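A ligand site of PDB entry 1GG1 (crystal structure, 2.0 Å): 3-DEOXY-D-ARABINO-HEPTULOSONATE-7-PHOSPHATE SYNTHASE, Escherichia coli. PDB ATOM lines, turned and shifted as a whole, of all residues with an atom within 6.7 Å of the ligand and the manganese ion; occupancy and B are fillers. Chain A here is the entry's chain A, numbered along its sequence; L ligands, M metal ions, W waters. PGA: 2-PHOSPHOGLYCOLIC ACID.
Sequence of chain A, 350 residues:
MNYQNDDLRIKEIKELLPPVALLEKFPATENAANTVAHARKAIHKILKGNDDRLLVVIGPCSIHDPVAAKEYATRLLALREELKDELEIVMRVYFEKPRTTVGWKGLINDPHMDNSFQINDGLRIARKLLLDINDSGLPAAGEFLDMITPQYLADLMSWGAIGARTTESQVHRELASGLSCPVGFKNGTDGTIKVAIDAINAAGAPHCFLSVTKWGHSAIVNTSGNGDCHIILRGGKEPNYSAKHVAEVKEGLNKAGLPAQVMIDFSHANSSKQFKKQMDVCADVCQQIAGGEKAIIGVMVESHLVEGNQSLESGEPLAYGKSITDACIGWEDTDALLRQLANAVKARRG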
ATOM      1  N   PRO A  60      31.774  20.187 -21.584  1.00  0.00           N
ATOM      2  CA  PRO A  60      32.342  20.801 -20.387  1.00  0.00           C
ATOM      3  C   PRO A  60      31.296  21.166 -19.341  1.00  0.00           C
ATOM      4  O   PRO A  60      30.086  21.255 -19.646  1.00  0.00           O
ATOM      5  CB  PRO A  60      33.046  22.038 -20.933  1.00  0.00           C
ATOM      6  CG  PRO A  60      33.350  21.667 -22.368  1.00  0.00           C
ATOM      7  CD  PRO A  60      32.066  21.015 -22.769  1.00  0.00           C
ATOM      8  N   CYS A  61      31.769  21.381 -18.111  1.00  0.00           N
ATOM      9  CA  CYS A  61      30.902  21.804 -17.015  1.00  0.00           C
ATOM     10  C   CYS A  61      30.407  23.208 -17.372  1.00  0.00           C
ATOM     11  O   CYS A  61      29.260  23.553 -17.096  1.00  0.00           O
ATOM     12  CB  CYS A  61      31.686  21.809 -15.688  1.00  0.00           C
ATOM     13  SG  CYS A  61      30.830  22.551 -14.251  1.00  0.00           S
ATOM     14  N   SER A  62      31.256  24.008 -17.997  1.00  0.00           N
ATOM     15  CA  SER A  62      30.872  25.368 -18.392  1.00  0.00           C
ATOM     16  C   SER A  62      31.769  25.869 -19.526  1.00  0.00           C
ATOM     17  O   SER A  62      32.965  25.592 -19.528  1.00  0.00           O
ATOM     18  CB  SER A  62      31.016  26.313 -17.198  1.00  0.00           C
ATOM     19  OG  SER A  62      32.350  26.306 -16.725  1.00  0.00           O
ATOM     20  N   ARG A  92      27.111  19.748 -24.401  1.00  0.00           N
ATOM     21  CA  ARG A  92      26.841  20.569 -23.216  1.00  0.00           C
ATOM     22  C   ARG A  92      27.469  21.930 -23.498  1.00  0.00           C
ATOM     23  O   ARG A  92      28.685  22.057 -23.568  1.00  0.00           O
ATOM     24  CB  ARG A  92      27.514  20.017 -21.953  1.00  0.00           C
ATOM     25  CG  ARG A  92      26.763  18.893 -21.257  1.00  0.00           C
ATOM     26  CD  ARG A  92      27.459  18.479 -19.947  1.00  0.00           C
ATOM     27  NE  ARG A  92      27.688  19.632 -19.076  1.00  0.00           N
ATOM     28  CZ  ARG A  92      27.214  19.762 -17.825  1.00  0.00           C
ATOM     29  NH1 ARG A  92      26.460  18.808 -17.269  1.00  0.00           N
ATOM     30  NH2 ARG A  92      27.488  20.839 -17.119  1.00  0.00           N
ATOM     31  N   TYR A  94      26.972  25.044 -21.600  1.00  0.00           N
ATOM     32  CA  TYR A  94      26.470  25.746 -20.425  1.00  0.00           C
ATOM     33  C   TYR A  94      27.077  27.132 -20.212  1.00  0.00           C
ATOM     34  O   TYR A  94      28.281  27.266 -19.996  1.00  0.00           O
ATOM     35  CB  TYR A  94      26.718  24.910 -19.166  1.00  0.00           C
ATOM     36  CG  TYR A  94      25.771  23.730 -18.999  1.00  0.00           C
ATOM     37  CD1 TYR A  94      25.441  22.923 -20.076  1.00  0.00           C
ATOM     38  CD2 TYR A  94      25.237  23.420 -17.741  1.00  0.00           C
ATOM     39  CE1 TYR A  94      24.608  21.828 -19.921  1.00  0.00           C
ATOM     40  CE2 TYR A  94      24.399  22.319 -17.574  1.00  0.00           C
ATOM     41  CZ  TYR A  94      24.095  21.538 -18.670  1.00  0.00           C
ATOM     42  OH  TYR A  94      23.262  20.452 -18.519  1.00  0.00           O
ATOM     43  N   LYS A  97      26.121  29.143 -14.489  1.00  0.00           N
ATOM     44  CA  LYS A  97      26.456  28.229 -13.407  1.00  0.00           C
ATOM     45  C   LYS A  97      25.945  28.669 -12.050  1.00  0.00           C
ATOM     46  O   LYS A  97      26.287  29.747 -11.562  1.00  0.00           O
ATOM     47  CB  LYS A  97      27.970  28.063 -13.318  1.00  0.00           C
ATOM     48  CG  LYS A  97      28.593  27.435 -14.559  1.00  0.00           C
ATOM     49  CD  LYS A  97      28.892  25.958 -14.368  1.00  0.00           C
ATOM     50  CE  LYS A  97      27.635  25.163 -14.401  1.00  0.00           C
ATOM     51  NZ  LYS A  97      27.836  23.723 -14.703  1.00  0.00           N
ATOM     52  N   PRO A  98      25.098  27.823 -11.407  1.00  0.00           N
ATOM     53  CA  PRO A  98      24.571  28.172 -10.088  1.00  0.00           C
ATOM     54  C   PRO A  98      25.665  27.837  -9.070  1.00  0.00           C
ATOM     55  O   PRO A  98      26.287  26.774  -9.135  1.00  0.00           O
ATOM     56  CB  PRO A  98      23.354  27.258  -9.966  1.00  0.00           C
ATOM     57  CG  PRO A  98      23.821  26.009 -10.646  1.00  0.00           C
ATOM     58  CD  PRO A  98      24.523  26.556 -11.892  1.00  0.00           C
ATOM     59  N   GLU A 143      21.848  24.621 -19.086  1.00  0.00           N
ATOM     60  CA  GLU A 143      21.010  24.743 -17.907  1.00  0.00           C
ATOM     61  C   GLU A 143      20.273  26.086 -17.970  1.00  0.00           C
ATOM     62  O   GLU A 143      20.868  27.140 -18.180  1.00  0.00           O
ATOM     63  CB  GLU A 143      21.811  24.684 -16.607  1.00  0.00           C
ATOM     64  CG  GLU A 143      20.847  24.783 -15.397  1.00  0.00           C
ATOM     65  CD  GLU A 143      21.513  24.776 -14.038  1.00  0.00           C
ATOM     66  OE1 GLU A 143      22.606  24.196 -13.901  1.00  0.00           O
ATOM     67  OE2 GLU A 143      20.906  25.343 -13.085  1.00  0.00           O
ATOM     68  N   ALA A 161      18.441  21.706 -19.083  1.00  0.00           N
ATOM     69  CA  ALA A 161      18.452  21.144 -17.741  1.00  0.00           C
ATOM     70  C   ALA A 161      18.034  22.153 -16.668  1.00  0.00           C
ATOM     71  O   ALA A 161      18.265  23.356 -16.800  1.00  0.00           O
ATOM     72  CB  ALA A 161      19.848  20.617 -17.414  1.00  0.00           C
ATOM     73  N   ILE A 162      17.364  21.667 -15.622  1.00  0.00           N
ATOM     74  CA  ILE A 162      17.000  22.517 -14.493  1.00  0.00           C
ATOM     75  C   ILE A 162      17.870  21.928 -13.392  1.00  0.00           C
ATOM     76  O   ILE A 162      17.780  20.731 -13.090  1.00  0.00           O
ATOM     77  CB  ILE A 162      15.492  22.404 -14.066  1.00  0.00           C
ATOM     78  CG1 ILE A 162      14.538  22.870 -15.171  1.00  0.00           C
ATOM     79  CG2 ILE A 162      15.168  23.271 -12.844  1.00  0.00           C
ATOM     80  CD1 ILE A 162      14.756  24.325 -15.592  1.00  0.00           C
ATOM     81  N   GLY A 163      18.726  22.770 -12.832  1.00  0.00           N
ATOM     82  CA  GLY A 163      19.631  22.353 -11.788  1.00  0.00           C
ATOM     83  C   GLY A 163      19.004  21.801 -10.507  1.00  0.00           C
ATOM     84  O   GLY A 163      17.875  22.143 -10.132  1.00  0.00           O
ATOM     85  N   ALA A 164      19.760  20.947  -9.818  1.00  0.00           N
ATOM     86  CA  ALA A 164      19.285  20.338  -8.582  1.00  0.00           C
ATOM     87  C   ALA A 164      18.801  21.365  -7.568  1.00  0.00           C
ATOM     88  O   ALA A 164      17.942  21.076  -6.714  1.00  0.00           O
ATOM     89  CB  ALA A 164      20.392  19.511  -7.960  1.00  0.00           C
ATOM     90  N   ARG A 165      19.357  22.571  -7.639  1.00  0.00           N
ATOM     91  CA  ARG A 165      19.044  23.633  -6.683  1.00  0.00           C
ATOM     92  C   ARG A 165      17.799  24.403  -7.034  1.00  0.00           C
ATOM     93  O   ARG A 165      17.360  25.207  -6.229  1.00  0.00           O
ATOM     94  CB  ARG A 165      20.219  24.612  -6.535  1.00  0.00           C
ATOM     95  CG  ARG A 165      21.489  23.926  -6.003  1.00  0.00           C
ATOM     96  CD  ARG A 165      22.752  24.796  -6.105  1.00  0.00           C
ATOM     97  NE  ARG A 165      23.950  23.963  -5.856  1.00  0.00           N
ATOM     98  CZ  ARG A 165      24.396  23.004  -6.672  1.00  0.00           C
ATOM     99  NH1 ARG A 165      23.765  22.732  -7.817  1.00  0.00           N
ATOM    100  NH2 ARG A 165      25.459  22.290  -6.330  1.00  0.00           N
ATOM    101  N   THR A 166      17.276  24.178  -8.230  1.00  0.00           N
ATOM    102  CA  THR A 166      16.083  24.882  -8.696  1.00  0.00           C
ATOM    103  C   THR A 166      14.983  23.952  -9.212  1.00  0.00           C
ATOM    104  O   THR A 166      13.958  24.417  -9.670  1.00  0.00           O
ATOM    105  CB  THR A 166      16.427  25.878  -9.815  1.00  0.00           C
ATOM    106  OG1 THR A 166      17.378  25.309 -10.718  1.00  0.00           O
ATOM    107  CG2 THR A 166      17.014  27.172  -9.210  1.00  0.00           C
ATOM    108  N   LYS A 186      16.874  17.707 -12.553  1.00  0.00           N
ATOM    109  CA  LYS A 186      17.750  16.979 -11.666  1.00  0.00           C
ATOM    110  C   LYS A 186      17.109  16.749 -10.306  1.00  0.00           C
ATOM    111  O   LYS A 186      16.320  17.581  -9.836  1.00  0.00           O
ATOM    112  CB  LYS A 186      19.055  17.755 -11.496  1.00  0.00           C
ATOM    113  CG  LYS A 186      19.835  17.844 -12.816  1.00  0.00           C
ATOM    114  CD  LYS A 186      21.286  18.080 -12.525  1.00  0.00           C
ATOM    115  CE  LYS A 186      22.209  17.519 -13.620  1.00  0.00           C
ATOM    116  NZ  LYS A 186      23.591  17.703 -13.105  1.00  0.00           N
ATOM    117  N   ASN A 187      17.444  15.637  -9.665  1.00  0.00           N
ATOM    118  CA  ASN A 187      16.918  15.386  -8.338  1.00  0.00           C
ATOM    119  C   ASN A 187      17.608  16.368  -7.391  1.00  0.00           C
ATOM    120  O   ASN A 187      18.634  16.964  -7.755  1.00  0.00           O
ATOM    121  CB  ASN A 187      17.148  13.916  -7.908  1.00  0.00           C
ATOM    122  CG  ASN A 187      18.638  13.524  -7.846  1.00  0.00           C
ATOM    123  OD1 ASN A 187      19.095  12.677  -8.625  1.00  0.00           O
ATOM    124  ND2 ASN A 187      19.379  14.098  -6.898  1.00  0.00           N
ATOM    125  N   THR A 189      19.719  18.291  -4.357  1.00  0.00           N
ATOM    126  CA  THR A 189      21.127  18.140  -3.982  1.00  0.00           C
ATOM    127  C   THR A 189      21.313  17.104  -2.869  1.00  0.00           C
ATOM    128  O   THR A 189      22.349  16.465  -2.794  1.00  0.00           O
ATOM    129  CB  THR A 189      21.754  19.506  -3.577  1.00  0.00           C
ATOM    130  OG1 THR A 189      20.958  20.139  -2.580  1.00  0.00           O
ATOM    131  CG2 THR A 189      21.882  20.432  -4.801  1.00  0.00           C
ATOM    132  N   ARG A 234      21.316  12.475 -10.432  1.00  0.00           N
ATOM    133  CA  ARG A 234      22.625  13.062 -10.250  1.00  0.00           C
ATOM    134  C   ARG A 234      23.234  12.841  -8.882  1.00  0.00           C
ATOM    135  O   ARG A 234      24.205  13.496  -8.502  1.00  0.00           O
ATOM    136  CB  ARG A 234      22.577  14.565 -10.581  1.00  0.00           C
ATOM    137  CG  ARG A 234      21.465  15.399  -9.866  1.00  0.00           C
ATOM    138  CD  ARG A 234      21.896  15.784  -8.479  1.00  0.00           C
ATOM    139  NE  ARG A 234      22.953  16.784  -8.511  1.00  0.00           N
ATOM    140  CZ  ARG A 234      23.702  17.098  -7.458  1.00  0.00           C
ATOM    141  NH1 ARG A 234      23.504  16.485  -6.310  1.00  0.00           N
ATOM    142  NH2 ARG A 234      24.639  18.024  -7.559  1.00  0.00           N
ATOM    143  N   ASP A 265      23.219  11.156 -14.792  1.00  0.00           N
ATOM    144  CA  ASP A 265      24.371  12.043 -14.845  1.00  0.00           C
ATOM    145  C   ASP A 265      25.511  11.270 -14.224  1.00  0.00           C
ATOM    146  O   ASP A 265      25.480  10.920 -13.050  1.00  0.00           O
ATOM    147  CB  ASP A 265      24.068  13.320 -14.051  1.00  0.00           C
ATOM    148  CG  ASP A 265      25.209  14.299 -14.035  1.00  0.00           C
ATOM    149  OD1 ASP A 265      26.259  14.033 -14.647  1.00  0.00           O
ATOM    150  OD2 ASP A 265      25.056  15.362 -13.387  1.00  0.00           O
ATOM    151  N   SER A 267      28.312  12.372 -13.623  1.00  0.00           N
ATOM    152  CA  SER A 267      29.146  13.275 -12.829  1.00  0.00           C
ATOM    153  C   SER A 267      28.531  13.806 -11.534  1.00  0.00           C
ATOM    154  O   SER A 267      27.554  13.259 -11.023  1.00  0.00           O
ATOM    155  CB  SER A 267      29.570  14.459 -13.699  1.00  0.00           C
ATOM    156  OG  SER A 267      30.618  15.183 -13.100  1.00  0.00           O
ATOM    157  N   HIS A 268      29.140  14.859 -10.996  1.00  0.00           N
ATOM    158  CA  HIS A 268      28.684  15.479  -9.761  1.00  0.00           C
ATOM    159  C   HIS A 268      28.565  14.515  -8.579  1.00  0.00           C
ATOM    160  O   HIS A 268      29.540  13.856  -8.225  1.00  0.00           O
ATOM    161  CB  HIS A 268      27.339  16.182 -10.001  1.00  0.00           C
ATOM    162  CG  HIS A 268      27.383  17.180 -11.118  1.00  0.00           C
ATOM    163  ND1 HIS A 268      26.938  16.886 -12.387  1.00  0.00           N
ATOM    164  CD2 HIS A 268      27.882  18.436 -11.169  1.00  0.00           C
ATOM    165  CE1 HIS A 268      27.164  17.911 -13.182  1.00  0.00           C
ATOM    166  NE2 HIS A 268      27.740  18.871 -12.469  1.00  0.00           N
ATOM    167  N   ALA A 269      27.383  14.448  -7.982  1.00  0.00           N
ATOM    168  CA  ALA A 269      27.173  13.595  -6.812  1.00  0.00           C
ATOM    169  C   ALA A 269      27.251  12.115  -7.124  1.00  0.00           C
ATOM    170  O   ALA A 269      27.444  11.318  -6.222  1.00  0.00           O
ATOM    171  CB  ALA A 269      25.840  13.926  -6.150  1.00  0.00           C
ATOM    172  N   MET A 300      24.374  11.895 -19.014  1.00  0.00           N
ATOM    173  CA  MET A 300      24.981  13.209 -19.033  1.00  0.00           C
ATOM    174  C   MET A 300      26.380  13.009 -18.509  1.00  0.00           C
ATOM    175  O   MET A 300      26.580  12.349 -17.482  1.00  0.00           O
ATOM    176  CB  MET A 300      24.191  14.170 -18.132  1.00  0.00           C
ATOM    177  CG  MET A 300      24.829  15.559 -17.914  1.00  0.00           C
ATOM    178  SD  MET A 300      23.816  16.638 -16.837  1.00  0.00           S
ATOM    179  CE  MET A 300      22.472  17.023 -17.953  1.00  0.00           C
ATOM    180  N   GLU A 302      30.433  15.035 -18.037  1.00  0.00           N
ATOM    181  CA  GLU A 302      31.255  16.224 -18.037  1.00  0.00           C
ATOM    182  C   GLU A 302      32.638  15.902 -18.598  1.00  0.00           C
ATOM    183  O   GLU A 302      33.486  15.348 -17.893  1.00  0.00           O
ATOM    184  CB  GLU A 302      31.372  16.795 -16.618  1.00  0.00           C
ATOM    185  CG  GLU A 302      30.079  17.527 -16.196  1.00  0.00           C
ATOM    186  CD  GLU A 302      30.175  18.253 -14.874  1.00  0.00           C
ATOM    187  OE1 GLU A 302      29.755  19.432 -14.829  1.00  0.00           O
ATOM    188  OE2 GLU A 302      30.642  17.652 -13.879  1.00  0.00           O
ATOM    189  N   THR A 325      35.567  25.054 -13.851  1.00  0.00           N
ATOM    190  CA  THR A 325      34.552  24.791 -12.843  1.00  0.00           C
ATOM    191  C   THR A 325      34.706  23.375 -12.246  1.00  0.00           C
ATOM    192  O   THR A 325      35.574  23.158 -11.399  1.00  0.00           O
ATOM    193  CB  THR A 325      33.118  24.992 -13.389  1.00  0.00           C
ATOM    194  OG1 THR A 325      33.036  24.450 -14.711  1.00  0.00           O
ATOM    195  CG2 THR A 325      32.782  26.478 -13.446  1.00  0.00           C
ATOM    196  N   ASP A 326      33.872  22.427 -12.666  1.00  0.00           N
ATOM    197  CA  ASP A 326      33.987  21.055 -12.146  1.00  0.00           C
ATOM    198  C   ASP A 326      34.977  20.297 -13.039  1.00  0.00           C
ATOM    199  O   ASP A 326      35.100  20.615 -14.219  1.00  0.00           O
ATOM    200  CB  ASP A 326      32.629  20.307 -12.161  1.00  0.00           C
ATOM    201  CG  ASP A 326      31.615  20.870 -11.134  1.00  0.00           C
ATOM    202  OD1 ASP A 326      32.014  21.324 -10.028  1.00  0.00           O
ATOM    203  OD2 ASP A 326      30.388  20.829 -11.437  1.00  0.00           O
HETATM  204  P   PGA L   1      23.638  20.103 -10.663  1.00  0.00           P
HETATM  205  O1P PGA L   1      24.236  20.059 -12.192  1.00  0.00           O
HETATM  206  O2P PGA L   1      24.734  20.594  -9.762  1.00  0.00           O
HETATM  207  O3P PGA L   1      22.468  21.045 -10.751  1.00  0.00           O
HETATM  208  O4P PGA L   1      23.247  18.674 -10.407  1.00  0.00           O
HETATM  209  C2  PGA L   1      25.212  21.015 -12.625  1.00  0.00           C
HETATM  210  C1  PGA L   1      25.780  20.728 -14.005  1.00  0.00           C
HETATM  211  O1  PGA L   1      25.224  20.113 -14.936  1.00  0.00           O
HETATM  212  O2  PGA L   1      26.944  21.125 -14.233  1.00  0.00           O
HETATM  213 MN    MN M   1      29.064  20.672 -13.184  1.00  0.00          MN
HETATM  214  O   HOH W   1      26.533  20.508  -8.174  1.00  0.00           O
HETATM  215  O   HOH W   2      22.978  19.689 -15.851  1.00  0.00           O
HETATM  216  O   HOH W   3      21.719  23.270  -9.223  1.00  0.00           O
HETATM  217  O   HOH W   4      22.187  21.262 -13.877  1.00  0.00           O
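NH1 of Arg 92 lies within salt-bridge range of O1 of the ligand.
The guanidinium group (NE) of Arg 234 is in salt-bridge range of an oxygen (O4P) of the ligand, 2.7 Å away.
NZ of Lys 97 sits close to O2 of the ligand (2.8 Å).
O2P of the ligand is in salt-bridge range of NH1 of Arg 165 (3.0 Å).
An oxygen (O3P) of the ligand lies within hydrogen-bond range of the backbone NH (N) of Ala 164 (2.9 Å).
The side-chain amino group of Lys 186 lies within salt-bridge range of an oxygen (O4P) of the ligand.
The side-chain carboxylate of Glu 143 sits at hydrogen-bond distance from the backbone NH of Gly 163.
A ring nitrogen (ND1) of His 268 lies within hydrogen-bond range of the side-chain carboxylate (OD2) of Asp 265, 2.6 Å away.
N of Lys 186 sits at hydrogen-bond distance from O of Ile 162, 3.2 Å away.
OE1 of Glu 302 sits close to NH2 of Arg 92 (3.5 Å).
SG of Cys 61 sits close to OG1 of Thr 325 (2.9 Å).
The backbone carbonyl oxygen (O) of Cys 61 is in hydrogen-bond range of the side-chain amino group (NZ) of Lys 97.
OD1 of Asn 187 lies within hydrogen-bond range of N of Arg 234 (2.9 Å).
The guanidinium group of Arg 92 lies within hydrogen-bond range of the backbone carbonyl oxygen of Pro 60, 3.0 Å away.
Merely in contact with the ligand: Gly 163 (3.3 Å) and Tyr 94 (3.5 Å).
Hydrophobic or aromatic side chains within 4 Å of the ligand: Tyr 94, Ala 164 and His 268.
Within 4 Å of the ligand: Arg 92, Tyr 94, Lys 97, Gly 163, Ala 164, Arg 165, Lys 186, Arg 234, His 268 and Glu 302.
Merely in contact with the manganese ion: Lys 97.
Within 4 Å of the manganese ion: Cys 61, Lys 97, His 268, Glu 302 and Asp 326.
OE1 of Glu 302 is bound to the manganese ion.
The side-chain carboxylate (OD2) of Asp 326 is bound to the manganese ion (2.2 Å).
NE2 of His 268 is bound to the manganese ion (2.3 Å).
The manganese ion is bound by O2 of the ligand, at 2.4 Å.
The manganese ion is bound by SG of Cys 61.
Water W1 lies within hydrogen-bond range of O2P of the ligand (2.4 Å), NH2 of Arg 165 (2.8 Å) and NH2 of Arg 234 (3.2 Å).
Water W2 lies within hydrogen-bond range of O1 of the ligand, OH of Tyr 94, SD of Met 300 and NZ of Lys 186.
Water W3 lies within hydrogen-bond range of the guanidinium group of Arg 165, an oxygen (O3P) of the ligand and the backbone NH of Ala 164.
Water W4 bridges O1P of the ligand (2.9 Å) and OE1 of Glu 143 (3.0 Å).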
